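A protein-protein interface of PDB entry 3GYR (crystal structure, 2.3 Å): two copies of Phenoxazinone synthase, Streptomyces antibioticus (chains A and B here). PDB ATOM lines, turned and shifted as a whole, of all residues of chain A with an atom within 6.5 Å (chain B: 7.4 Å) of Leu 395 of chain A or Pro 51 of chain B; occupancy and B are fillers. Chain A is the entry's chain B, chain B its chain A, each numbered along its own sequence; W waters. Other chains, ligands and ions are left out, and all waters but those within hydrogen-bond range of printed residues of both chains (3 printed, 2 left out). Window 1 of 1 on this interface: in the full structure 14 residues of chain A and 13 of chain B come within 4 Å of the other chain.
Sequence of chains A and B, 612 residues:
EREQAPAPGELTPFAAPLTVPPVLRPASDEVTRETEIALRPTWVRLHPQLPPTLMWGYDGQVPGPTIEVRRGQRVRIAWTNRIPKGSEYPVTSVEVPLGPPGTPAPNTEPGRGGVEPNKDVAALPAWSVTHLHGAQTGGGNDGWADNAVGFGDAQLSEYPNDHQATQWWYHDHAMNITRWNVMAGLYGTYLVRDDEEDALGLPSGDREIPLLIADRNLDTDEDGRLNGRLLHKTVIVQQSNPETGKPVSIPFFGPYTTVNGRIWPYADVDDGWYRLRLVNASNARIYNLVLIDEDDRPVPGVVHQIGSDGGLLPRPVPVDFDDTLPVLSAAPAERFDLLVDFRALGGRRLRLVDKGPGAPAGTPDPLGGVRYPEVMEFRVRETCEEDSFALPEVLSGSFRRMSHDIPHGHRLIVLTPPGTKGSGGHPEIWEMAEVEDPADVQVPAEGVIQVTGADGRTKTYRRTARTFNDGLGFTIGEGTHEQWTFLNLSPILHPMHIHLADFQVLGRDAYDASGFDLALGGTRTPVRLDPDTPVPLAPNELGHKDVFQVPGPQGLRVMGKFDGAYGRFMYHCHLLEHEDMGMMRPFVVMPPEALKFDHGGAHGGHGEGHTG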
ATOM      1  N   GLU A 196      -5.175  29.187 -11.583  1.00  0.00           N
ATOM      2  CA  GLU A 196      -3.832  28.708 -11.797  1.00  0.00           C
ATOM      3  C   GLU A 196      -2.911  29.900 -11.939  1.00  0.00           C
ATOM      4  O   GLU A 196      -1.915  30.025 -11.240  1.00  0.00           O
ATOM      5  CB  GLU A 196      -3.737  27.784 -13.015  1.00  0.00           C
ATOM      6  CG  GLU A 196      -2.332  27.221 -13.185  1.00  0.00           C
ATOM      7  CD  GLU A 196      -2.200  26.266 -14.348  1.00  0.00           C
ATOM      8  OE1 GLU A 196      -3.069  26.318 -15.235  1.00  0.00           O
ATOM      9  OE2 GLU A 196      -1.231  25.450 -14.374  1.00  0.00           O
ATOM     10  N   ALA A 199      -2.271  31.872  -8.785  1.00  0.00           N
ATOM     11  CA  ALA A 199      -1.423  31.237  -7.810  1.00  0.00           C
ATOM     12  C   ALA A 199       0.061  31.442  -8.093  1.00  0.00           C
ATOM     13  O   ALA A 199       0.905  31.135  -7.255  1.00  0.00           O
ATOM     14  CB  ALA A 199      -1.761  29.800  -7.688  1.00  0.00           C
ATOM     15  N   LEU A 200       0.388  31.975  -9.272  1.00  0.00           N
ATOM     16  CA  LEU A 200       1.774  32.367  -9.552  1.00  0.00           C
ATOM     17  C   LEU A 200       2.182  33.715  -8.916  1.00  0.00           C
ATOM     18  O   LEU A 200       3.359  34.086  -8.918  1.00  0.00           O
ATOM     19  CB  LEU A 200       2.059  32.323 -11.059  1.00  0.00           C
ATOM     20  CG  LEU A 200       2.246  30.902 -11.638  1.00  0.00           C
ATOM     21  CD1 LEU A 200       2.052  30.928 -13.115  1.00  0.00           C
ATOM     22  CD2 LEU A 200       3.596  30.283 -11.330  1.00  0.00           C
ATOM     23  N   LEU A 202       1.872  36.827 -10.084  1.00  0.00           N
ATOM     24  CA  LEU A 202       2.658  37.584 -11.071  1.00  0.00           C
ATOM     25  C   LEU A 202       2.504  39.099 -10.869  1.00  0.00           C
ATOM     26  O   LEU A 202       1.510  39.541 -10.295  1.00  0.00           O
ATOM     27  CB  LEU A 202       2.237  37.203 -12.496  1.00  0.00           C
ATOM     28  CG  LEU A 202       2.341  35.725 -12.904  1.00  0.00           C
ATOM     29  CD1 LEU A 202       1.560  35.469 -14.184  1.00  0.00           C
ATOM     30  CD2 LEU A 202       3.799  35.229 -13.036  1.00  0.00           C
ATOM     31  N   GLN A 305       9.943  34.811 -21.219  1.00  0.00           N
ATOM     32  CA  GLN A 305       8.581  34.499 -21.674  1.00  0.00           C
ATOM     33  C   GLN A 305       7.840  33.458 -20.793  1.00  0.00           C
ATOM     34  O   GLN A 305       8.368  32.428 -20.473  1.00  0.00           O
ATOM     35  CB  GLN A 305       8.581  34.076 -23.134  1.00  0.00           C
ATOM     36  CG  GLN A 305       7.179  33.865 -23.681  1.00  0.00           C
ATOM     37  CD  GLN A 305       7.171  33.668 -25.178  1.00  0.00           C
ATOM     38  OE1 GLN A 305       8.126  34.014 -25.871  1.00  0.00           O
ATOM     39  NE2 GLN A 305       6.089  33.107 -25.686  1.00  0.00           N
ATOM     40  N   ILE A 306       6.598  33.724 -20.422  1.00  0.00           N
ATOM     41  CA  ILE A 306       5.872  32.814 -19.539  1.00  0.00           C
ATOM     42  C   ILE A 306       4.523  32.360 -20.099  1.00  0.00           C
ATOM     43  O   ILE A 306       3.838  31.534 -19.482  1.00  0.00           O
ATOM     44  CB  ILE A 306       5.676  33.399 -18.110  1.00  0.00           C
ATOM     45  CG1 ILE A 306       4.993  34.785 -18.160  1.00  0.00           C
ATOM     46  CG2 ILE A 306       7.026  33.492 -17.405  1.00  0.00           C
ATOM     47  CD1 ILE A 306       4.091  35.082 -16.937  1.00  0.00           C
ATOM     48  N   GLY A 307       4.160  32.894 -21.268  1.00  0.00           N
ATOM     49  CA  GLY A 307       2.868  32.597 -21.909  1.00  0.00           C
ATOM     50  C   GLY A 307       2.910  32.776 -23.419  1.00  0.00           C
ATOM     51  O   GLY A 307       3.821  33.424 -23.952  1.00  0.00           O
ATOM     52  N   LEU A 312      -0.284  30.116 -20.227  1.00  0.00           N
ATOM     53  CA  LEU A 312       1.020  29.882 -19.591  1.00  0.00           C
ATOM     54  C   LEU A 312       1.827  28.782 -20.301  1.00  0.00           C
ATOM     55  O   LEU A 312       1.316  27.724 -20.649  1.00  0.00           O
ATOM     56  CB  LEU A 312       0.828  29.532 -18.111  1.00  0.00           C
ATOM     57  CG  LEU A 312       0.201  30.569 -17.169  1.00  0.00           C
ATOM     58  CD1 LEU A 312      -0.148  29.941 -15.851  1.00  0.00           C
ATOM     59  CD2 LEU A 312       1.147  31.730 -16.897  1.00  0.00           C
ATOM     60  N   LEU A 313       3.105  29.035 -20.503  1.00  0.00           N
ATOM     61  CA  LEU A 313       3.985  28.016 -21.033  1.00  0.00           C
ATOM     62  C   LEU A 313       4.172  26.940 -19.978  1.00  0.00           C
ATOM     63  O   LEU A 313       3.987  27.210 -18.807  1.00  0.00           O
ATOM     64  CB  LEU A 313       5.338  28.650 -21.352  1.00  0.00           C
ATOM     65  CG  LEU A 313       5.365  29.638 -22.523  1.00  0.00           C
ATOM     66  CD1 LEU A 313       6.794  30.015 -22.822  1.00  0.00           C
ATOM     67  CD2 LEU A 313       4.736  29.045 -23.739  1.00  0.00           C
ATOM     68  N   PRO A 314       4.594  25.727 -20.377  1.00  0.00           N
ATOM     69  CA  PRO A 314       4.902  24.780 -19.318  1.00  0.00           C
ATOM     70  C   PRO A 314       6.107  25.235 -18.468  1.00  0.00           C
ATOM     71  O   PRO A 314       6.115  25.027 -17.237  1.00  0.00           O
ATOM     72  CB  PRO A 314       5.200  23.481 -20.074  1.00  0.00           C
ATOM     73  CG  PRO A 314       5.577  23.927 -21.461  1.00  0.00           C
ATOM     74  CD  PRO A 314       4.773  25.147 -21.722  1.00  0.00           C
ATOM     75  N   ARG A 315       7.098  25.840 -19.123  1.00  0.00           N
ATOM     76  CA  ARG A 315       8.250  26.413 -18.435  1.00  0.00           C
ATOM     77  C   ARG A 315       8.532  27.848 -18.944  1.00  0.00           C
ATOM     78  O   ARG A 315       8.334  28.144 -20.122  1.00  0.00           O
ATOM     79  CB  ARG A 315       9.502  25.540 -18.638  1.00  0.00           C
ATOM     80  CG  ARG A 315       9.340  24.134 -18.121  1.00  0.00           C
ATOM     81  CD  ARG A 315      10.480  23.211 -18.523  1.00  0.00           C
ATOM     82  NE  ARG A 315      10.297  21.904 -17.896  1.00  0.00           N
ATOM     83  CZ  ARG A 315      11.272  21.063 -17.514  1.00  0.00           C
ATOM     84  NH1 ARG A 315      12.563  21.365 -17.661  1.00  0.00           N
ATOM     85  NH2 ARG A 315      10.937  19.909 -16.954  1.00  0.00           N
ATOM     86  N   PRO A 316       9.091  28.699 -18.069  1.00  0.00           N
ATOM     87  CA  PRO A 316       9.599  30.002 -18.492  1.00  0.00           C
ATOM     88  C   PRO A 316      10.702  29.827 -19.533  1.00  0.00           C
ATOM     89  O   PRO A 316      11.528  28.942 -19.398  1.00  0.00           O
ATOM     90  CB  PRO A 316      10.219  30.563 -17.207  1.00  0.00           C
ATOM     91  CG  PRO A 316       9.796  29.647 -16.112  1.00  0.00           C
ATOM     92  CD  PRO A 316       9.594  28.332 -16.743  1.00  0.00           C
ATOM     93  N   LEU A 339       7.803  38.447 -18.645  1.00  0.00           N
ATOM     94  CA  LEU A 339       8.236  39.125 -17.409  1.00  0.00           C
ATOM     95  C   LEU A 339       9.527  39.812 -17.705  1.00  0.00           C
ATOM     96  O   LEU A 339      10.366  39.311 -18.481  1.00  0.00           O
ATOM     97  CB  LEU A 339       8.424  38.181 -16.245  1.00  0.00           C
ATOM     98  CG  LEU A 339       7.198  37.347 -15.865  1.00  0.00           C
ATOM     99  CD1 LEU A 339       7.539  36.407 -14.733  1.00  0.00           C
ATOM    100  CD2 LEU A 339       6.013  38.235 -15.490  1.00  0.00           C
ATOM    101  N   LEU A 391      10.555  33.200  -9.834  1.00  0.00           N
ATOM    102  CA  LEU A 391      10.111  32.544 -11.070  1.00  0.00           C
ATOM    103  C   LEU A 391      10.422  31.068 -11.020  1.00  0.00           C
ATOM    104  O   LEU A 391      11.587  30.685 -11.046  1.00  0.00           O
ATOM    105  CB  LEU A 391      10.740  33.198 -12.311  1.00  0.00           C
ATOM    106  CG  LEU A 391      10.232  32.814 -13.713  1.00  0.00           C
ATOM    107  CD1 LEU A 391       8.726  32.901 -13.905  1.00  0.00           C
ATOM    108  CD2 LEU A 391      10.928  33.697 -14.745  1.00  0.00           C
ATOM    109  N   PRO A 392       9.391  30.219 -10.902  1.00  0.00           N
ATOM    110  CA  PRO A 392       9.739  28.811 -10.792  1.00  0.00           C
ATOM    111  C   PRO A 392      10.135  28.163 -12.133  1.00  0.00           C
ATOM    112  O   PRO A 392       9.728  28.626 -13.214  1.00  0.00           O
ATOM    113  CB  PRO A 392       8.455  28.172 -10.277  1.00  0.00           C
ATOM    114  CG  PRO A 392       7.347  29.073 -10.738  1.00  0.00           C
ATOM    115  CD  PRO A 392       7.949  30.463 -10.699  1.00  0.00           C
ATOM    116  N   GLU A 393      10.824  27.027 -12.035  1.00  0.00           N
ATOM    117  CA  GLU A 393      11.465  26.395 -13.169  1.00  0.00           C
ATOM    118  C   GLU A 393      10.471  25.712 -14.076  1.00  0.00           C
ATOM    119  O   GLU A 393      10.627  25.728 -15.286  1.00  0.00           O
ATOM    120  CB  GLU A 393      12.508  25.413 -12.687  1.00  0.00           C
ATOM    121  CG  GLU A 393      13.596  26.125 -11.991  1.00  0.00           C
ATOM    122  CD  GLU A 393      14.841  26.119 -12.788  1.00  0.00           C
ATOM    123  OE1 GLU A 393      15.755  25.394 -12.355  1.00  0.00           O
ATOM    124  OE2 GLU A 393      14.888  26.759 -13.869  1.00  0.00           O
ATOM    125  N   VAL A 394       9.504  25.049 -13.467  1.00  0.00           N
ATOM    126  CA  VAL A 394       8.281  24.687 -14.119  1.00  0.00           C
ATOM    127  C   VAL A 394       7.230  25.701 -13.668  1.00  0.00           C
ATOM    128  O   VAL A 394       7.219  26.136 -12.512  1.00  0.00           O
ATOM    129  CB  VAL A 394       7.859  23.272 -13.700  1.00  0.00           C
ATOM    130  CG1 VAL A 394       6.580  22.860 -14.403  1.00  0.00           C
ATOM    131  CG2 VAL A 394       9.009  22.253 -13.960  1.00  0.00           C
ATOM    132  N   LEU A 395       6.307  26.023 -14.564  1.00  0.00           N
ATOM    133  CA  LEU A 395       5.480  27.190 -14.436  1.00  0.00           C
ATOM    134  C   LEU A 395       3.994  26.845 -14.334  1.00  0.00           C
ATOM    135  O   LEU A 395       3.241  27.452 -13.544  1.00  0.00           O
ATOM    136  CB  LEU A 395       5.737  28.087 -15.659  1.00  0.00           C
ATOM    137  CG  LEU A 395       5.122  29.488 -15.587  1.00  0.00           C
ATOM    138  CD1 LEU A 395       5.827  30.403 -14.563  1.00  0.00           C
ATOM    139  CD2 LEU A 395       5.114  30.092 -16.985  1.00  0.00           C
ATOM    140  N   SER A 396       3.550  25.927 -15.180  1.00  0.00           N
ATOM    141  CA  SER A 396       2.151  25.526 -15.223  1.00  0.00           C
ATOM    142  C   SER A 396       2.044  24.063 -14.897  1.00  0.00           C
ATOM    143  O   SER A 396       2.621  23.232 -15.591  1.00  0.00           O
ATOM    144  CB  SER A 396       1.508  25.795 -16.605  1.00  0.00           C
ATOM    145  OG  SER A 396       0.251  25.121 -16.779  1.00  0.00           O
ATOM    146  N   GLY A 397       1.284  23.765 -13.841  1.00  0.00           N
ATOM    147  CA  GLY A 397       0.956  22.384 -13.480  1.00  0.00           C
ATOM    148  C   GLY A 397      -0.236  21.830 -14.231  1.00  0.00           C
ATOM    149  O   GLY A 397      -0.433  20.640 -14.209  1.00  0.00           O
ATOM    150  N   TRP B  43      -6.205  25.949  -6.874  1.00  0.00           N
ATOM    151  CA  TRP B  43      -4.797  25.875  -7.238  1.00  0.00           C
ATOM    152  C   TRP B  43      -3.938  26.392  -6.096  1.00  0.00           C
ATOM    153  O   TRP B  43      -4.167  27.480  -5.590  1.00  0.00           O
ATOM    154  CB  TRP B  43      -4.542  26.655  -8.534  1.00  0.00           C
ATOM    155  CG  TRP B  43      -5.042  25.919  -9.697  1.00  0.00           C
ATOM    156  CD1 TRP B  43      -6.303  25.978 -10.215  1.00  0.00           C
ATOM    157  CD2 TRP B  43      -4.356  24.883 -10.409  1.00  0.00           C
ATOM    158  NE1 TRP B  43      -6.429  25.070 -11.257  1.00  0.00           N
ATOM    159  CE2 TRP B  43      -5.256  24.377 -11.385  1.00  0.00           C
ATOM    160  CE3 TRP B  43      -3.074  24.329 -10.314  1.00  0.00           C
ATOM    161  CZ2 TRP B  43      -4.904  23.361 -12.289  1.00  0.00           C
ATOM    162  CZ3 TRP B  43      -2.713  23.319 -11.238  1.00  0.00           C
ATOM    163  CH2 TRP B  43      -3.635  22.847 -12.203  1.00  0.00           C
ATOM    164  N   VAL B  44      -2.967  25.590  -5.672  1.00  0.00           N
ATOM    165  CA  VAL B  44      -2.268  25.830  -4.423  1.00  0.00           C
ATOM    166  C   VAL B  44      -0.773  25.951  -4.664  1.00  0.00           C
ATOM    167  O   VAL B  44      -0.166  25.106  -5.319  1.00  0.00           O
ATOM    168  CB  VAL B  44      -2.530  24.669  -3.442  1.00  0.00           C
ATOM    169  CG1 VAL B  44      -1.755  24.867  -2.161  1.00  0.00           C
ATOM    170  CG2 VAL B  44      -4.036  24.568  -3.152  1.00  0.00           C
ATOM    171  N   ARG B  45      -0.165  26.983  -4.099  1.00  0.00           N
ATOM    172  CA  ARG B  45       1.255  27.169  -4.283  1.00  0.00           C
ATOM    173  C   ARG B  45       1.947  26.490  -3.123  1.00  0.00           C
ATOM    174  O   ARG B  45       2.174  27.112  -2.075  1.00  0.00           O
ATOM    175  CB  ARG B  45       1.630  28.668  -4.364  1.00  0.00           C
ATOM    176  CG  ARG B  45       3.072  28.896  -4.830  1.00  0.00           C
ATOM    177  CD  ARG B  45       3.236  28.624  -6.316  1.00  0.00           C
ATOM    178  NE  ARG B  45       4.524  29.061  -6.846  1.00  0.00           N
ATOM    179  CZ  ARG B  45       4.841  30.329  -7.135  1.00  0.00           C
ATOM    180  NH1 ARG B  45       3.949  31.314  -6.982  1.00  0.00           N
ATOM    181  NH2 ARG B  45       6.065  30.610  -7.593  1.00  0.00           N
ATOM    182  N   LEU B  46       2.277  25.216  -3.288  1.00  0.00           N
ATOM    183  CA  LEU B  46       3.025  24.527  -2.223  1.00  0.00           C
ATOM    184  C   LEU B  46       4.345  25.223  -1.840  1.00  0.00           C
ATOM    185  O   LEU B  46       4.768  25.204  -0.683  1.00  0.00           O
ATOM    186  CB  LEU B  46       3.277  23.078  -2.607  1.00  0.00           C
ATOM    187  CG  LEU B  46       2.062  22.167  -2.337  1.00  0.00           C
ATOM    188  CD1 LEU B  46       2.330  20.761  -2.822  1.00  0.00           C
ATOM    189  CD2 LEU B  46       1.719  22.161  -0.797  1.00  0.00           C
ATOM    190  N   HIS B  47       4.984  25.875  -2.812  1.00  0.00           N
ATOM    191  CA  HIS B  47       6.324  26.392  -2.610  1.00  0.00           C
ATOM    192  C   HIS B  47       6.683  27.361  -3.735  1.00  0.00           C
ATOM    193  O   HIS B  47       6.485  27.047  -4.922  1.00  0.00           O
ATOM    194  CB  HIS B  47       7.332  25.235  -2.577  1.00  0.00           C
ATOM    195  CG  HIS B  47       8.679  25.630  -2.065  1.00  0.00           C
ATOM    196  ND1 HIS B  47       9.592  26.316  -2.837  1.00  0.00           N
ATOM    197  CD2 HIS B  47       9.237  25.515  -0.830  1.00  0.00           C
ATOM    198  CE1 HIS B  47      10.673  26.563  -2.117  1.00  0.00           C
ATOM    199  NE2 HIS B  47      10.477  26.104  -0.892  1.00  0.00           N
ATOM    200  N   PRO B  48       7.292  28.500  -3.380  1.00  0.00           N
ATOM    201  CA  PRO B  48       7.658  29.514  -4.406  1.00  0.00           C
ATOM    202  C   PRO B  48       8.399  28.911  -5.604  1.00  0.00           C
ATOM    203  O   PRO B  48       8.313  29.446  -6.713  1.00  0.00           O
ATOM    204  CB  PRO B  48       8.585  30.481  -3.645  1.00  0.00           C
ATOM    205  CG  PRO B  48       8.165  30.364  -2.227  1.00  0.00           C
ATOM    206  CD  PRO B  48       7.709  28.907  -2.017  1.00  0.00           C
ATOM    207  N   GLN B  49       9.064  27.777  -5.392  1.00  0.00           N
ATOM    208  CA  GLN B  49       9.892  27.168  -6.422  1.00  0.00           C
ATOM    209  C   GLN B  49       9.181  26.104  -7.251  1.00  0.00           C
ATOM    210  O   GLN B  49       9.761  25.539  -8.143  1.00  0.00           O
ATOM    211  CB  GLN B  49      11.145  26.579  -5.782  1.00  0.00           C
ATOM    212  CG  GLN B  49      12.084  27.601  -5.230  1.00  0.00           C
ATOM    213  CD  GLN B  49      13.352  26.968  -4.651  1.00  0.00           C
ATOM    214  OE1 GLN B  49      13.395  26.534  -3.486  1.00  0.00           O
ATOM    215  NE2 GLN B  49      14.382  26.901  -5.470  1.00  0.00           N
ATOM    216  N   LEU B  50       7.926  25.817  -6.919  1.00  0.00           N
ATOM    217  CA  LEU B  50       7.075  24.940  -7.712  1.00  0.00           C
ATOM    218  C   LEU B  50       6.050  25.765  -8.512  1.00  0.00           C
ATOM    219  O   LEU B  50       5.742  26.907  -8.146  1.00  0.00           O
ATOM    220  CB  LEU B  50       6.322  23.983  -6.781  1.00  0.00           C
ATOM    221  CG  LEU B  50       7.136  22.921  -6.017  1.00  0.00           C
ATOM    222  CD1 LEU B  50       6.301  22.349  -4.865  1.00  0.00           C
ATOM    223  CD2 LEU B  50       7.605  21.790  -6.920  1.00  0.00           C
ATOM    224  N   PRO B  51       5.463  25.164  -9.566  1.00  0.00           N
ATOM    225  CA  PRO B  51       4.236  25.727 -10.149  1.00  0.00           C
ATOM    226  C   PRO B  51       3.058  25.454  -9.222  1.00  0.00           C
ATOM    227  O   PRO B  51       3.203  24.671  -8.281  1.00  0.00           O
ATOM    228  CB  PRO B  51       4.059  24.920 -11.434  1.00  0.00           C
ATOM    229  CG  PRO B  51       4.645  23.561 -11.105  1.00  0.00           C
ATOM    230  CD  PRO B  51       5.812  23.847 -10.154  1.00  0.00           C
ATOM    231  N   PRO B  52       1.896  26.083  -9.486  1.00  0.00           N
ATOM    232  CA  PRO B  52       0.715  25.819  -8.705  1.00  0.00           C
ATOM    233  C   PRO B  52       0.351  24.357  -8.776  1.00  0.00           C
ATOM    234  O   PRO B  52       0.729  23.671  -9.742  1.00  0.00           O
ATOM    235  CB  PRO B  52      -0.350  26.683  -9.390  1.00  0.00           C
ATOM    236  CG  PRO B  52       0.428  27.816  -9.983  1.00  0.00           C
ATOM    237  CD  PRO B  52       1.641  27.124 -10.501  1.00  0.00           C
ATOM    238  N   THR B  53      -0.280  23.874  -7.702  1.00  0.00           N
ATOM    239  CA  THR B  53      -0.674  22.487  -7.550  1.00  0.00           C
ATOM    240  C   THR B  53      -2.212  22.393  -7.523  1.00  0.00           C
ATOM    241  O   THR B  53      -2.886  23.144  -6.785  1.00  0.00           O
ATOM    242  CB  THR B  53      -0.072  21.922  -6.253  1.00  0.00           C
ATOM    243  OG1 THR B  53       1.354  21.960  -6.349  1.00  0.00           O
ATOM    244  CG2 THR B  53      -0.523  20.471  -6.008  1.00  0.00           C
ATOM    245  N   LEU B  54      -2.766  21.546  -8.397  1.00  0.00           N
ATOM    246  CA  LEU B  54      -4.209  21.245  -8.384  1.00  0.00           C
ATOM    247  C   LEU B  54      -4.561  20.440  -7.124  1.00  0.00           C
ATOM    248  O   LEU B  54      -3.966  19.369  -6.882  1.00  0.00           O
ATOM    249  CB  LEU B  54      -4.602  20.419  -9.632  1.00  0.00           C
ATOM    250  CG  LEU B  54      -6.064  19.935  -9.799  1.00  0.00           C
ATOM    251  CD1 LEU B  54      -7.038  21.066  -9.699  1.00  0.00           C
ATOM    252  CD2 LEU B  54      -6.267  19.187 -11.110  1.00  0.00           C
ATOM    253  N   ASP B 221       8.913  15.970 -14.004  1.00  0.00           N
ATOM    254  CA  ASP B 221       8.932  15.914 -15.432  1.00  0.00           C
ATOM    255  C   ASP B 221      10.034  14.981 -15.798  1.00  0.00           C
ATOM    256  O   ASP B 221      10.811  14.478 -14.959  1.00  0.00           O
ATOM    257  CB  ASP B 221       9.252  17.270 -16.065  1.00  0.00           C
ATOM    258  CG  ASP B 221       8.062  18.207 -16.101  1.00  0.00           C
ATOM    259  OD1 ASP B 221       6.904  17.743 -15.978  1.00  0.00           O
ATOM    260  OD2 ASP B 221       8.294  19.424 -16.261  1.00  0.00           O
ATOM    261  N   LEU B 226      10.750  18.768 -10.624  1.00  0.00           N
ATOM    262  CA  LEU B 226       9.519  18.716  -9.865  1.00  0.00           C
ATOM    263  C   LEU B 226       8.407  19.523 -10.543  1.00  0.00           C
ATOM    264  O   LEU B 226       8.633  20.666 -10.980  1.00  0.00           O
ATOM    265  CB  LEU B 226       9.768  19.295  -8.473  1.00  0.00           C
ATOM    266  CG  LEU B 226      10.581  18.449  -7.511  1.00  0.00           C
ATOM    267  CD1 LEU B 226      11.061  19.343  -6.395  1.00  0.00           C
ATOM    268  CD2 LEU B 226       9.716  17.325  -6.956  1.00  0.00           C
ATOM    269  N   ASN B 227       7.203  18.962 -10.630  1.00  0.00           N
ATOM    270  CA  ASN B 227       6.172  19.670 -11.364  1.00  0.00           C
ATOM    271  C   ASN B 227       4.930  20.065 -10.557  1.00  0.00           C
ATOM    272  O   ASN B 227       3.949  20.554 -11.117  1.00  0.00           O
ATOM    273  CB  ASN B 227       5.784  18.889 -12.607  1.00  0.00           C
ATOM    274  CG  ASN B 227       5.235  17.532 -12.276  1.00  0.00           C
ATOM    275  OD1 ASN B 227       4.499  17.355 -11.291  1.00  0.00           O
ATOM    276  ND2 ASN B 227       5.592  16.546 -13.098  1.00  0.00           N
ATOM    277  N   GLY B 228       4.953  19.811  -9.259  1.00  0.00           N
ATOM    278  CA  GLY B 228       3.899  20.299  -8.380  1.00  0.00           C
ATOM    279  C   GLY B 228       2.694  19.394  -8.314  1.00  0.00           C
ATOM    280  O   GLY B 228       1.791  19.624  -7.509  1.00  0.00           O
ATOM    281  N   ARG B 229       2.669  18.347  -9.131  1.00  0.00           N
ATOM    282  CA  ARG B 229       1.518  17.450  -9.106  1.00  0.00           C
ATOM    283  C   ARG B 229       1.634  16.507  -7.914  1.00  0.00           C
ATOM    284  O   ARG B 229       2.697  15.915  -7.688  1.00  0.00           O
ATOM    285  CB  ARG B 229       1.414  16.622 -10.386  1.00  0.00           C
ATOM    286  CG  ARG B 229       1.253  17.385 -11.682  1.00  0.00           C
ATOM    287  CD  ARG B 229       0.808  16.369 -12.676  1.00  0.00           C
ATOM    288  NE  ARG B 229       1.078  16.732 -14.058  1.00  0.00           N
ATOM    289  CZ  ARG B 229       1.766  15.980 -14.918  1.00  0.00           C
ATOM    290  NH1 ARG B 229       2.299  14.821 -14.522  1.00  0.00           N
ATOM    291  NH2 ARG B 229       1.939  16.398 -16.171  1.00  0.00           N
HETATM  292  O   HOH W   1      12.057  26.044  -9.597  1.00  0.00           O
HETATM  293  O   HOH W   2      -7.014  27.186 -13.456  1.00  0.00           O
HETATM  294  O   HOH W   3       9.169  24.380 -10.583  1.00  0.00           O
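The side-chain carboxylate of Glu 196 of chain A lies within hydrogen-bond range of the side-chain hydroxyl of Ser 396 of chain A.
The backbone NH (N) of Leu 395 of chain A is in hydrogen-bond range of the backbone carbonyl oxygen (O) of Pro 314 of chain A, at 2.9 Å.
O of Pro 314 of chain A sits at hydrogen-bond distance from N of Ser 396 of chain A, 3.4 Å away.
Hydrophobic or aromatic side chains of chain A that line the printed part of chain B: Ala 199, Leu 200, Pro 392 and Val 394.
Of the 17 printed residues of chain B, 9 touch a printed residue of chain A.
Among the printed residues, 20 pairs touch across the chains.
The guanidinium group (NH1) of Arg 45 of chain B is in hydrogen-bond range of the backbone carbonyl oxygen (O) of Ala 199 of chain A, at 3.1 Å.
NH1 of Arg 45 of chain B is in hydrogen-bond range of O of Leu 200 of chain A, 3.4 Å away.
OD2 of Asp 221 of chain B is in salt-bridge range of NH2 of Arg 315 of chain A (2.8 Å).
No position is printed for both chains.
Among the printed residues, merely in contact across the chains: Leu 395 of chain A with Pro 51 of chain B (3.4 Å), Val 394 of chain A with Leu 226 of chain B (3.4 Å), Leu 395 of chain A with Pro 52 of chain B (3.5 Å), Glu 196 of chain A with Pro 52 of chain B (3.5 Å), Val 394 of chain A with Pro 51 of chain B (3.6 Å), Pro 392 of chain A with Gln 49 of chain B (3.6 Å), Pro 392 of chain A with Arg 45 of chain B (3.6 Å), Glu 196 of chain A with Trp 43 of chain B (3.7 Å), Pro 392 of chain A with Leu 50 of chain B (3.7 Å), Val 394 of chain A with Asp 221 of chain B (3.7 Å), Ala 199 of chain A with Pro 52 of chain B (3.7 Å), Pro 392 of chain A with Pro 48 of chain B (3.8 Å), Leu 200 of chain A with Pro 52 of chain B (3.8 Å), Gly 397 of chain A with Pro 51 of chain B (3.9 Å), Ser 396 of chain A with Pro 51 of chain B (3.9 Å), Ala 199 of chain A with Trp 43 of chain B (3.9 Å) and Gly 397 of chain A with Pro 52 of chain B (3.96 Å).
Water W3 lies within hydrogen-bond range of O of Gln 49 of chain B (2.8 Å), N of Val 394 of chain A (3.0 Å) and N of Glu 393 of chain A (3.4 Å).
Water W1 bridges the backbone carbonyl oxygen (O) of Gln 49 of chain B and the backbone NH (N) of Glu 393 of chain A.
Water W2 lies within hydrogen-bond range of NE1 of Trp 43 of chain B (3.1 Å) and N of Glu 196 of chain A (3.3 Å).
Of the printed residues of chain B, Arg 315 of chain A touches Asp 221 (2.8 Å).
Leu 391 of chain A touches none of the printed residues of chain B.
Of the printed residues of chain B, Pro 392 of chain A touches Arg 45, Pro 48, Gln 49 and Leu 50.
Leu 395 of chain A touches just these residues of chain B: Pro 51 (3.4 Å) and Pro 52 (3.5 Å).
Printed residues of chain A within 4 Å of Arg 45 of chain B: Ala 199, Leu 200 and Pro 392.
Of the printed residues of chain A, Gln 49 of chain B touches Pro 392.
The nearest residue of chain A that does not touch Pro 51 of chain B is Pro 392 of chain A (4.3 Å).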
